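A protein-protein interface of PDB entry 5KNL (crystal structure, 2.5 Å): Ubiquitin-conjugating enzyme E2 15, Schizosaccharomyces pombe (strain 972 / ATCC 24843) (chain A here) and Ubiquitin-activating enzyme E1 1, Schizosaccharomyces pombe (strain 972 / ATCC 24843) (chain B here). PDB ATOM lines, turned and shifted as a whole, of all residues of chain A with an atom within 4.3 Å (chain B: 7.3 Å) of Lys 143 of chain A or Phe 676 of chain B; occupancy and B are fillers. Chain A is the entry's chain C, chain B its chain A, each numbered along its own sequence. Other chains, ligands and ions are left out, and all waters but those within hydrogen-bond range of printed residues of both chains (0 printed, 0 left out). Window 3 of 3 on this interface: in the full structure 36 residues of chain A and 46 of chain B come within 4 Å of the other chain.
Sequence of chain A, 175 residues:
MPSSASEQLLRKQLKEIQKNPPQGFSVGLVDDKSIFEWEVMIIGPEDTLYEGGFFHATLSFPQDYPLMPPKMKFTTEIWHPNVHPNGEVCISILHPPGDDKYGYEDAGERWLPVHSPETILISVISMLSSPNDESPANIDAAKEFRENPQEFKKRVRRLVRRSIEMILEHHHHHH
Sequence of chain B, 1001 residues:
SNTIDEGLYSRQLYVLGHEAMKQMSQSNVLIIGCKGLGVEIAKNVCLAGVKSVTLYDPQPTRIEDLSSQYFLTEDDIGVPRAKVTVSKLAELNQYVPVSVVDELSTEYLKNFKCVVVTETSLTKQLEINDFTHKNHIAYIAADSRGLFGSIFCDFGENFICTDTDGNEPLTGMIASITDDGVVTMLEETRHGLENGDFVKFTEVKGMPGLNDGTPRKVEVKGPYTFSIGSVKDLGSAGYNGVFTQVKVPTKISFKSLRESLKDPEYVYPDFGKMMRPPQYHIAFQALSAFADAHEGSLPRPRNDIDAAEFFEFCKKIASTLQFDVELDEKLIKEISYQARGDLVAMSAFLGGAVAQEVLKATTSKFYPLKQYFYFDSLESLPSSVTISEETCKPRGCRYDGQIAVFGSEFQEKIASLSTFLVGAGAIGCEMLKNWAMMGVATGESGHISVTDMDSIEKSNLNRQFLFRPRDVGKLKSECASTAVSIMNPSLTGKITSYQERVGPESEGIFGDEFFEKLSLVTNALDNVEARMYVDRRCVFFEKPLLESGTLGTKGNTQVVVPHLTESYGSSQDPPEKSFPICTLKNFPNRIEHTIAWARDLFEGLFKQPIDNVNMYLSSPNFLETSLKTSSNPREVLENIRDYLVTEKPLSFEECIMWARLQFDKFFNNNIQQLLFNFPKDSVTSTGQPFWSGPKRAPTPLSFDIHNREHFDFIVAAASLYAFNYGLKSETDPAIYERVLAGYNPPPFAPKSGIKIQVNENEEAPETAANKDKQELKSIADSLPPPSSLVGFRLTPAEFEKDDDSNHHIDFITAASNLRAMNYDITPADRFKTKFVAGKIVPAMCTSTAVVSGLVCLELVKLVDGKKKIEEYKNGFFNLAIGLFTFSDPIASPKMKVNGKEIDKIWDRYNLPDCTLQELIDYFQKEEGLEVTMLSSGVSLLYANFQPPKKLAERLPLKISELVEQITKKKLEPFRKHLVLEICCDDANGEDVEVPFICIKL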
ATOM      1  N   ILE A 139      17.322 -33.367 -33.282  1.00  0.00           N
ATOM      2  CA  ILE A 139      17.079 -32.430 -32.190  1.00  0.00           C
ATOM      3  C   ILE A 139      18.368 -32.093 -31.448  1.00  0.00           C
ATOM      4  O   ILE A 139      18.648 -30.927 -31.170  1.00  0.00           O
ATOM      5  CB  ILE A 139      16.064 -33.000 -31.177  1.00  0.00           C
ATOM      6  CG1 ILE A 139      14.735 -33.318 -31.863  1.00  0.00           C
ATOM      7  CG2 ILE A 139      15.840 -32.024 -30.027  1.00  0.00           C
ATOM      8  CD1 ILE A 139      13.808 -34.148 -31.006  1.00  0.00           C
ATOM      9  N   ASP A 140      19.144 -33.122 -31.127  1.00  0.00           N
ATOM     10  CA  ASP A 140      20.398 -32.943 -30.405  1.00  0.00           C
ATOM     11  C   ASP A 140      21.372 -32.066 -31.188  1.00  0.00           C
ATOM     12  O   ASP A 140      22.023 -31.188 -30.621  1.00  0.00           O
ATOM     13  CB  ASP A 140      21.034 -34.303 -30.105  1.00  0.00           C
ATOM     14  CG  ASP A 140      20.231 -35.114 -29.104  1.00  0.00           C
ATOM     15  OD1 ASP A 140      19.618 -34.508 -28.199  1.00  0.00           O
ATOM     16  OD2 ASP A 140      20.209 -36.358 -29.224  1.00  0.00           O
ATOM     17  N   ALA A 141      21.461 -32.301 -32.492  1.00  0.00           N
ATOM     18  CA  ALA A 141      22.350 -31.522 -33.343  1.00  0.00           C
ATOM     19  C   ALA A 141      21.840 -30.095 -33.478  1.00  0.00           C
ATOM     20  O   ALA A 141      22.626 -29.150 -33.572  1.00  0.00           O
ATOM     21  CB  ALA A 141      22.477 -32.170 -34.712  1.00  0.00           C
ATOM     22  N   ALA A 142      20.520 -29.944 -33.480  1.00  0.00           N
ATOM     23  CA  ALA A 142      19.899 -28.637 -33.646  1.00  0.00           C
ATOM     24  C   ALA A 142      20.173 -27.742 -32.444  1.00  0.00           C
ATOM     25  O   ALA A 142      20.235 -26.520 -32.576  1.00  0.00           O
ATOM     26  CB  ALA A 142      18.403 -28.786 -33.864  1.00  0.00           C
ATOM     27  N   LYS A 143      20.332 -28.350 -31.271  1.00  0.00           N
ATOM     28  CA  LYS A 143      20.608 -27.586 -30.060  1.00  0.00           C
ATOM     29  C   LYS A 143      22.074 -27.198 -29.976  1.00  0.00           C
ATOM     30  O   LYS A 143      22.408 -26.038 -29.729  1.00  0.00           O
ATOM     31  CB  LYS A 143      20.234 -28.373 -28.804  1.00  0.00           C
ATOM     32  CG  LYS A 143      19.794 -27.477 -27.657  1.00  0.00           C
ATOM     33  CD  LYS A 143      20.324 -27.947 -26.311  1.00  0.00           C
ATOM     34  CE  LYS A 143      19.812 -29.319 -25.936  1.00  0.00           C
ATOM     35  NZ  LYS A 143      19.870 -29.529 -24.464  1.00  0.00           N
ATOM     36  N   GLU A 144      22.944 -28.181 -30.178  1.00  0.00           N
ATOM     37  CA  GLU A 144      24.379 -27.974 -30.053  1.00  0.00           C
ATOM     38  C   GLU A 144      24.839 -26.887 -31.018  1.00  0.00           C
ATOM     39  O   GLU A 144      25.733 -26.104 -30.705  1.00  0.00           O
ATOM     40  CB  GLU A 144      25.130 -29.282 -30.309  1.00  0.00           C
ATOM     41  CG  GLU A 144      26.444 -29.400 -29.548  1.00  0.00           C
ATOM     42  CD  GLU A 144      27.224 -30.647 -29.915  1.00  0.00           C
ATOM     43  OE1 GLU A 144      26.755 -31.410 -30.785  1.00  0.00           O
ATOM     44  OE2 GLU A 144      28.300 -30.874 -29.322  1.00  0.00           O
ATOM     45  N   PHE A 145      24.218 -26.847 -32.193  1.00  0.00           N
ATOM     46  CA  PHE A 145      24.538 -25.840 -33.200  1.00  0.00           C
ATOM     47  C   PHE A 145      24.134 -24.438 -32.744  1.00  0.00           C
ATOM     48  O   PHE A 145      24.621 -23.440 -33.277  1.00  0.00           O
ATOM     49  CB  PHE A 145      23.845 -26.177 -34.522  1.00  0.00           C
ATOM     50  CG  PHE A 145      24.169 -25.224 -35.639  1.00  0.00           C
ATOM     51  CD1 PHE A 145      25.370 -25.320 -36.322  1.00  0.00           C
ATOM     52  CD2 PHE A 145      23.274 -24.233 -36.005  1.00  0.00           C
ATOM     53  CE1 PHE A 145      25.671 -24.447 -37.349  1.00  0.00           C
ATOM     54  CE2 PHE A 145      23.570 -23.357 -37.032  1.00  0.00           C
ATOM     55  CZ  PHE A 145      24.770 -23.465 -37.704  1.00  0.00           C
ATOM     56  N   ARG A 146      23.253 -24.371 -31.749  1.00  0.00           N
ATOM     57  CA  ARG A 146      22.685 -23.104 -31.296  1.00  0.00           C
ATOM     58  C   ARG A 146      23.286 -22.630 -29.976  1.00  0.00           C
ATOM     59  O   ARG A 146      23.583 -21.447 -29.817  1.00  0.00           O
ATOM     60  CB  ARG A 146      21.167 -23.238 -31.148  1.00  0.00           C
ATOM     61  CG  ARG A 146      20.450 -21.946 -30.780  1.00  0.00           C
ATOM     62  CD  ARG A 146      18.967 -22.188 -30.527  1.00  0.00           C
ATOM     63  NE  ARG A 146      18.742 -23.071 -29.383  1.00  0.00           N
ATOM     64  CZ  ARG A 146      17.728 -23.927 -29.270  1.00  0.00           C
ATOM     65  NH1 ARG A 146      16.819 -24.035 -30.231  1.00  0.00           N
ATOM     66  NH2 ARG A 146      17.621 -24.683 -28.185  1.00  0.00           N
ATOM     67  N   GLU A 147      23.465 -23.553 -29.036  1.00  0.00           N
ATOM     68  CA  GLU A 147      23.859 -23.190 -27.678  1.00  0.00           C
ATOM     69  C   GLU A 147      25.365 -23.310 -27.442  1.00  0.00           C
ATOM     70  O   GLU A 147      25.906 -22.660 -26.548  1.00  0.00           O
ATOM     71  CB  GLU A 147      23.107 -24.058 -26.668  1.00  0.00           C
ATOM     72  CG  GLU A 147      21.606 -23.807 -26.650  1.00  0.00           C
ATOM     73  CD  GLU A 147      20.897 -24.557 -25.537  1.00  0.00           C
ATOM     74  OE1 GLU A 147      21.571 -25.304 -24.797  1.00  0.00           O
ATOM     75  OE2 GLU A 147      19.665 -24.397 -25.403  1.00  0.00           O
ATOM     76  N   ASN B 670       8.968 -37.642 -23.377  1.00  0.00           N
ATOM     77  CA  ASN B 670       9.485 -37.261 -24.685  1.00  0.00           C
ATOM     78  C   ASN B 670       9.160 -35.808 -25.002  1.00  0.00           C
ATOM     79  O   ASN B 670       9.915 -35.133 -25.701  1.00  0.00           O
ATOM     80  CB  ASN B 670       8.922 -38.173 -25.778  1.00  0.00           C
ATOM     81  CG  ASN B 670       7.412 -38.100 -25.879  1.00  0.00           C
ATOM     82  OD1 ASN B 670       6.728 -37.774 -24.910  1.00  0.00           O
ATOM     83  ND2 ASN B 670       6.884 -38.408 -27.056  1.00  0.00           N
ATOM     84  N   ILE B 671       8.035 -35.328 -24.480  1.00  0.00           N
ATOM     85  CA  ILE B 671       7.634 -33.941 -24.683  1.00  0.00           C
ATOM     86  C   ILE B 671       8.478 -33.026 -23.806  1.00  0.00           C
ATOM     87  O   ILE B 671       8.860 -31.936 -24.232  1.00  0.00           O
ATOM     88  CB  ILE B 671       6.136 -33.725 -24.377  1.00  0.00           C
ATOM     89  CG1 ILE B 671       5.270 -34.605 -25.285  1.00  0.00           C
ATOM     90  CG2 ILE B 671       5.752 -32.257 -24.544  1.00  0.00           C
ATOM     91  CD1 ILE B 671       5.460 -34.356 -26.777  1.00  0.00           C
ATOM     92  N   GLN B 672       8.765 -33.466 -22.585  1.00  0.00           N
ATOM     93  CA  GLN B 672       9.674 -32.730 -21.717  1.00  0.00           C
ATOM     94  C   GLN B 672      11.032 -32.624 -22.393  1.00  0.00           C
ATOM     95  O   GLN B 672      11.625 -31.548 -22.462  1.00  0.00           O
ATOM     96  CB  GLN B 672       9.823 -33.413 -20.359  1.00  0.00           C
ATOM     97  CG  GLN B 672       8.587 -33.373 -19.485  1.00  0.00           C
ATOM     98  CD  GLN B 672       8.838 -33.974 -18.116  1.00  0.00           C
ATOM     99  OE1 GLN B 672       9.868 -33.716 -17.493  1.00  0.00           O
ATOM    100  NE2 GLN B 672       7.902 -34.787 -17.644  1.00  0.00           N
ATOM    101  N   GLN B 673      11.510 -33.759 -22.896  1.00  0.00           N
ATOM    102  CA  GLN B 673      12.802 -33.833 -23.565  1.00  0.00           C
ATOM    103  C   GLN B 673      12.847 -32.914 -24.782  1.00  0.00           C
ATOM    104  O   GLN B 673      13.851 -32.248 -25.024  1.00  0.00           O
ATOM    105  CB  GLN B 673      13.101 -35.273 -23.980  1.00  0.00           C
ATOM    106  CG  GLN B 673      14.532 -35.500 -24.432  1.00  0.00           C
ATOM    107  CD  GLN B 673      15.528 -35.329 -23.305  1.00  0.00           C
ATOM    108  OE1 GLN B 673      15.476 -36.041 -22.301  1.00  0.00           O
ATOM    109  NE2 GLN B 673      16.441 -34.377 -23.460  1.00  0.00           N
ATOM    110  N   LEU B 674      11.762 -32.886 -25.549  1.00  0.00           N
ATOM    111  CA  LEU B 674      11.680 -32.018 -26.719  1.00  0.00           C
ATOM    112  C   LEU B 674      11.702 -30.561 -26.286  1.00  0.00           C
ATOM    113  O   LEU B 674      12.307 -29.715 -26.947  1.00  0.00           O
ATOM    114  CB  LEU B 674      10.411 -32.303 -27.528  1.00  0.00           C
ATOM    115  CG  LEU B 674      10.142 -31.368 -28.715  1.00  0.00           C
ATOM    116  CD1 LEU B 674      11.278 -31.415 -29.719  1.00  0.00           C
ATOM    117  CD2 LEU B 674       8.827 -31.711 -29.389  1.00  0.00           C
ATOM    118  N   LEU B 675      11.029 -30.274 -25.176  1.00  0.00           N
ATOM    119  CA  LEU B 675      10.971 -28.920 -24.641  1.00  0.00           C
ATOM    120  C   LEU B 675      12.309 -28.486 -24.060  1.00  0.00           C
ATOM    121  O   LEU B 675      12.664 -27.315 -24.132  1.00  0.00           O
ATOM    122  CB  LEU B 675       9.884 -28.815 -23.571  1.00  0.00           C
ATOM    123  CG  LEU B 675       8.437 -28.809 -24.065  1.00  0.00           C
ATOM    124  CD1 LEU B 675       7.490 -28.932 -22.889  1.00  0.00           C
ATOM    125  CD2 LEU B 675       8.124 -27.556 -24.869  1.00  0.00           C
ATOM    126  N   PHE B 676      13.053 -29.419 -23.477  1.00  0.00           N
ATOM    127  CA  PHE B 676      14.367 -29.083 -22.946  1.00  0.00           C
ATOM    128  C   PHE B 676      15.314 -28.727 -24.086  1.00  0.00           C
ATOM    129  O   PHE B 676      16.203 -27.892 -23.927  1.00  0.00           O
ATOM    130  CB  PHE B 676      14.943 -30.229 -22.117  1.00  0.00           C
ATOM    131  CG  PHE B 676      16.323 -29.953 -21.597  1.00  0.00           C
ATOM    132  CD1 PHE B 676      16.532 -28.959 -20.653  1.00  0.00           C
ATOM    133  CD2 PHE B 676      17.411 -30.675 -22.053  1.00  0.00           C
ATOM    134  CE1 PHE B 676      17.800 -28.696 -20.173  1.00  0.00           C
ATOM    135  CE2 PHE B 676      18.682 -30.415 -21.575  1.00  0.00           C
ATOM    136  CZ  PHE B 676      18.876 -29.425 -20.633  1.00  0.00           C
ATOM    137  N   ASN B 677      15.120 -29.368 -25.235  1.00  0.00           N
ATOM    138  CA  ASN B 677      15.918 -29.078 -26.419  1.00  0.00           C
ATOM    139  C   ASN B 677      15.427 -27.818 -27.120  1.00  0.00           C
ATOM    140  O   ASN B 677      16.213 -27.077 -27.712  1.00  0.00           O
ATOM    141  CB  ASN B 677      15.892 -30.260 -27.390  1.00  0.00           C
ATOM    142  CG  ASN B 677      16.610 -31.482 -26.844  1.00  0.00           C
ATOM    143  OD1 ASN B 677      17.838 -31.551 -26.861  1.00  0.00           O
ATOM    144  ND2 ASN B 677      15.845 -32.455 -26.368  1.00  0.00           N
ATOM    145  N   PHE B 678      14.120 -27.587 -27.047  1.00  0.00           N
ATOM    146  CA  PHE B 678      13.498 -26.410 -27.643  1.00  0.00           C
ATOM    147  C   PHE B 678      12.468 -25.831 -26.681  1.00  0.00           C
ATOM    148  O   PHE B 678      11.273 -26.095 -26.820  1.00  0.00           O
ATOM    149  CB  PHE B 678      12.835 -26.759 -28.976  1.00  0.00           C
ATOM    150  CG  PHE B 678      13.807 -27.022 -30.088  1.00  0.00           C
ATOM    151  CD1 PHE B 678      14.149 -26.017 -30.976  1.00  0.00           C
ATOM    152  CD2 PHE B 678      14.380 -28.273 -30.247  1.00  0.00           C
ATOM    153  CE1 PHE B 678      15.043 -26.252 -32.003  1.00  0.00           C
ATOM    154  CE2 PHE B 678      15.275 -28.513 -31.271  1.00  0.00           C
ATOM    155  CZ  PHE B 678      15.606 -27.501 -32.149  1.00  0.00           C
ATOM    156  N   PRO B 679      12.936 -25.061 -25.685  1.00  0.00           N
ATOM    157  CA  PRO B 679      12.060 -24.408 -24.705  1.00  0.00           C
ATOM    158  C   PRO B 679      10.919 -23.628 -25.347  1.00  0.00           C
ATOM    159  O   PRO B 679      10.993 -23.259 -26.521  1.00  0.00           O
ATOM    160  CB  PRO B 679      13.014 -23.475 -23.962  1.00  0.00           C
ATOM    161  CG  PRO B 679      14.318 -24.187 -24.004  1.00  0.00           C
ATOM    162  CD  PRO B 679      14.358 -24.913 -25.325  1.00  0.00           C
ATOM    163  N   LYS B 680       9.877 -23.373 -24.566  1.00  0.00           N
ATOM    164  CA  LYS B 680       8.650 -22.789 -25.083  1.00  0.00           C
ATOM    165  C   LYS B 680       8.890 -21.380 -25.624  1.00  0.00           C
ATOM    166  O   LYS B 680       8.147 -20.906 -26.484  1.00  0.00           O
ATOM    167  CB  LYS B 680       7.579 -22.774 -23.990  1.00  0.00           C
ATOM    168  CG  LYS B 680       6.177 -23.106 -24.482  1.00  0.00           C
ATOM    169  CD  LYS B 680       5.565 -24.246 -23.672  1.00  0.00           C
ATOM    170  CE  LYS B 680       4.191 -24.642 -24.197  1.00  0.00           C
ATOM    171  NZ  LYS B 680       3.269 -23.478 -24.344  1.00  0.00           N
ATOM    172  N   SER B 682      11.830 -20.402 -27.058  1.00  0.00           N
ATOM    173  CA  SER B 682      12.999 -20.467 -27.929  1.00  0.00           C
ATOM    174  C   SER B 682      12.862 -19.536 -29.129  1.00  0.00           C
ATOM    175  O   SER B 682      11.757 -19.135 -29.497  1.00  0.00           O
ATOM    176  CB  SER B 682      13.228 -21.898 -28.414  1.00  0.00           C
ATOM    177  OG  SER B 682      13.476 -22.766 -27.324  1.00  0.00           O
ATOM    178  N   ALA B 749      14.118 -36.968 -15.846  1.00  0.00           N
ATOM    179  CA  ALA B 749      14.708 -35.650 -16.035  1.00  0.00           C
ATOM    180  C   ALA B 749      15.278 -35.520 -17.449  1.00  0.00           C
ATOM    181  O   ALA B 749      15.968 -36.424 -17.922  1.00  0.00           O
ATOM    182  CB  ALA B 749      15.793 -35.406 -15.002  1.00  0.00           C
ATOM    183  N   PRO B 750      14.981 -34.401 -18.135  1.00  0.00           N
ATOM    184  CA  PRO B 750      15.540 -34.148 -19.471  1.00  0.00           C
ATOM    185  C   PRO B 750      17.069 -34.162 -19.495  1.00  0.00           C
ATOM    186  O   PRO B 750      17.700 -33.360 -18.807  1.00  0.00           O
ATOM    187  CB  PRO B 750      15.003 -32.757 -19.821  1.00  0.00           C
ATOM    188  CG  PRO B 750      13.758 -32.628 -19.040  1.00  0.00           C
ATOM    189  CD  PRO B 750      13.998 -33.367 -17.759  1.00  0.00           C
ATOM    190  N   LYS B 751      17.652 -35.069 -20.276  1.00  0.00           N
ATOM    191  CA  LYS B 751      19.103 -35.164 -20.389  1.00  0.00           C
ATOM    192  C   LYS B 751      19.652 -34.063 -21.287  1.00  0.00           C
ATOM    193  O   LYS B 751      18.917 -33.468 -22.074  1.00  0.00           O
ATOM    194  CB  LYS B 751      19.515 -36.522 -20.960  1.00  0.00           C
ATOM    195  CG  LYS B 751      19.438 -37.690 -19.993  1.00  0.00           C
ATOM    196  CD  LYS B 751      20.072 -38.939 -20.602  1.00  0.00           C
ATOM    197  CE  LYS B 751      19.307 -39.425 -21.832  1.00  0.00           C
ATOM    198  NZ  LYS B 751      19.898 -40.660 -22.421  1.00  0.00           N
ATOM    199  N   SER B 752      20.951 -33.810 -21.166  1.00  0.00           N
ATOM    200  CA  SER B 752      21.622 -32.788 -21.960  1.00  0.00           C
ATOM    201  C   SER B 752      22.285 -33.405 -23.187  1.00  0.00           C
ATOM    202  O   SER B 752      21.986 -34.539 -23.561  1.00  0.00           O
ATOM    203  CB  SER B 752      22.658 -32.051 -21.111  1.00  0.00           C
ATOM    204  OG  SER B 752      23.056 -30.840 -21.729  1.00  0.00           O
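Of the 16 printed residues of chain B, 4 touch a printed residue of chain A. Hydrophobic or aromatic side chains of chain B that line the printed part of chain A: Leu 674, Phe 676 and Phe 678. Of the 9 printed residues of chain A, 5 touch a printed residue of chain B. Printed residues of chain A that touch a printed residue of chain B: Ile 139, Asp 140, Ala 142, Lys 143 and Arg 146. Hydrophobic or aromatic side chains of chain A within 4 Å of the printed part of chain B: Ile 139 and Ala 142. Along chain A the printed residues that touch a printed residue of chain B span positions 139 to 146. Among the printed residues, no Asp or Glu carboxylate lies within 4 Å of a Lys or Arg side-chain nitrogen of the other chain.
Printed residues of chain B within 4 Å of Ala 142 of chain A: Phe 678 (3.5 Å). Lys 143 of chain A touches just these residues of chain B: Phe 676 and Asn 677. Of the printed residues of chain B, Arg 146 of chain A touches Asn 677 (2.8 Å) and Phe 678 (3.3 Å). Phe 676 of chain B touches just one residue of chain A: Lys 143. The nearest residue of chain B that does not touch Lys 143 of chain A is Ser 752 of chain B (4.4 Å). The nearest printed residue of chain A that does not touch Phe 676 of chain B is Glu 147 of chain A (5.1 Å). The nearest printed residue of chain A that does not touch Leu 674 of chain B is Arg 146 of chain A (7.4 Å).
ND2 of Asn 677 of chain B is in hydrogen-bond range of O of Gln 673 of chain B, 2.4 Å away. The side-chain carboxylate (OE2) of Glu 147 of chain A lies within salt-bridge range of the guanidinium group (NH2) of Arg 146 of chain A, 3.5 Å away.
The backbone carbonyl oxygen (O) of Asn 677 of chain B lies within hydrogen-bond range of the guanidinium group (NH2) of Arg 146 of chain A.
Leu 674 of chain B touches Ile 139 of chain A. Asn 677 of chain B touches Ile 139 of chain A. CE2 of Phe 678 of chain B touches CG2 of Ile 139 of chain A (3.8 Å). OD1 of Asp 140 of chain A touches OD1 of Asn 677 of chain B, at 3.7 Å. Phe 678 of chain B touches Ala 142 of chain A (CZ to CB, 3.5 Å). Lys 143 of chain A touches Phe 676 of chain B (NZ to CE2, 3.2 Å). Lys 143 of chain A touches Asn 677 of chain B. CE1 of Phe 678 of chain B touches NH1 of Arg 146 of chain A, at 3.3 Å.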
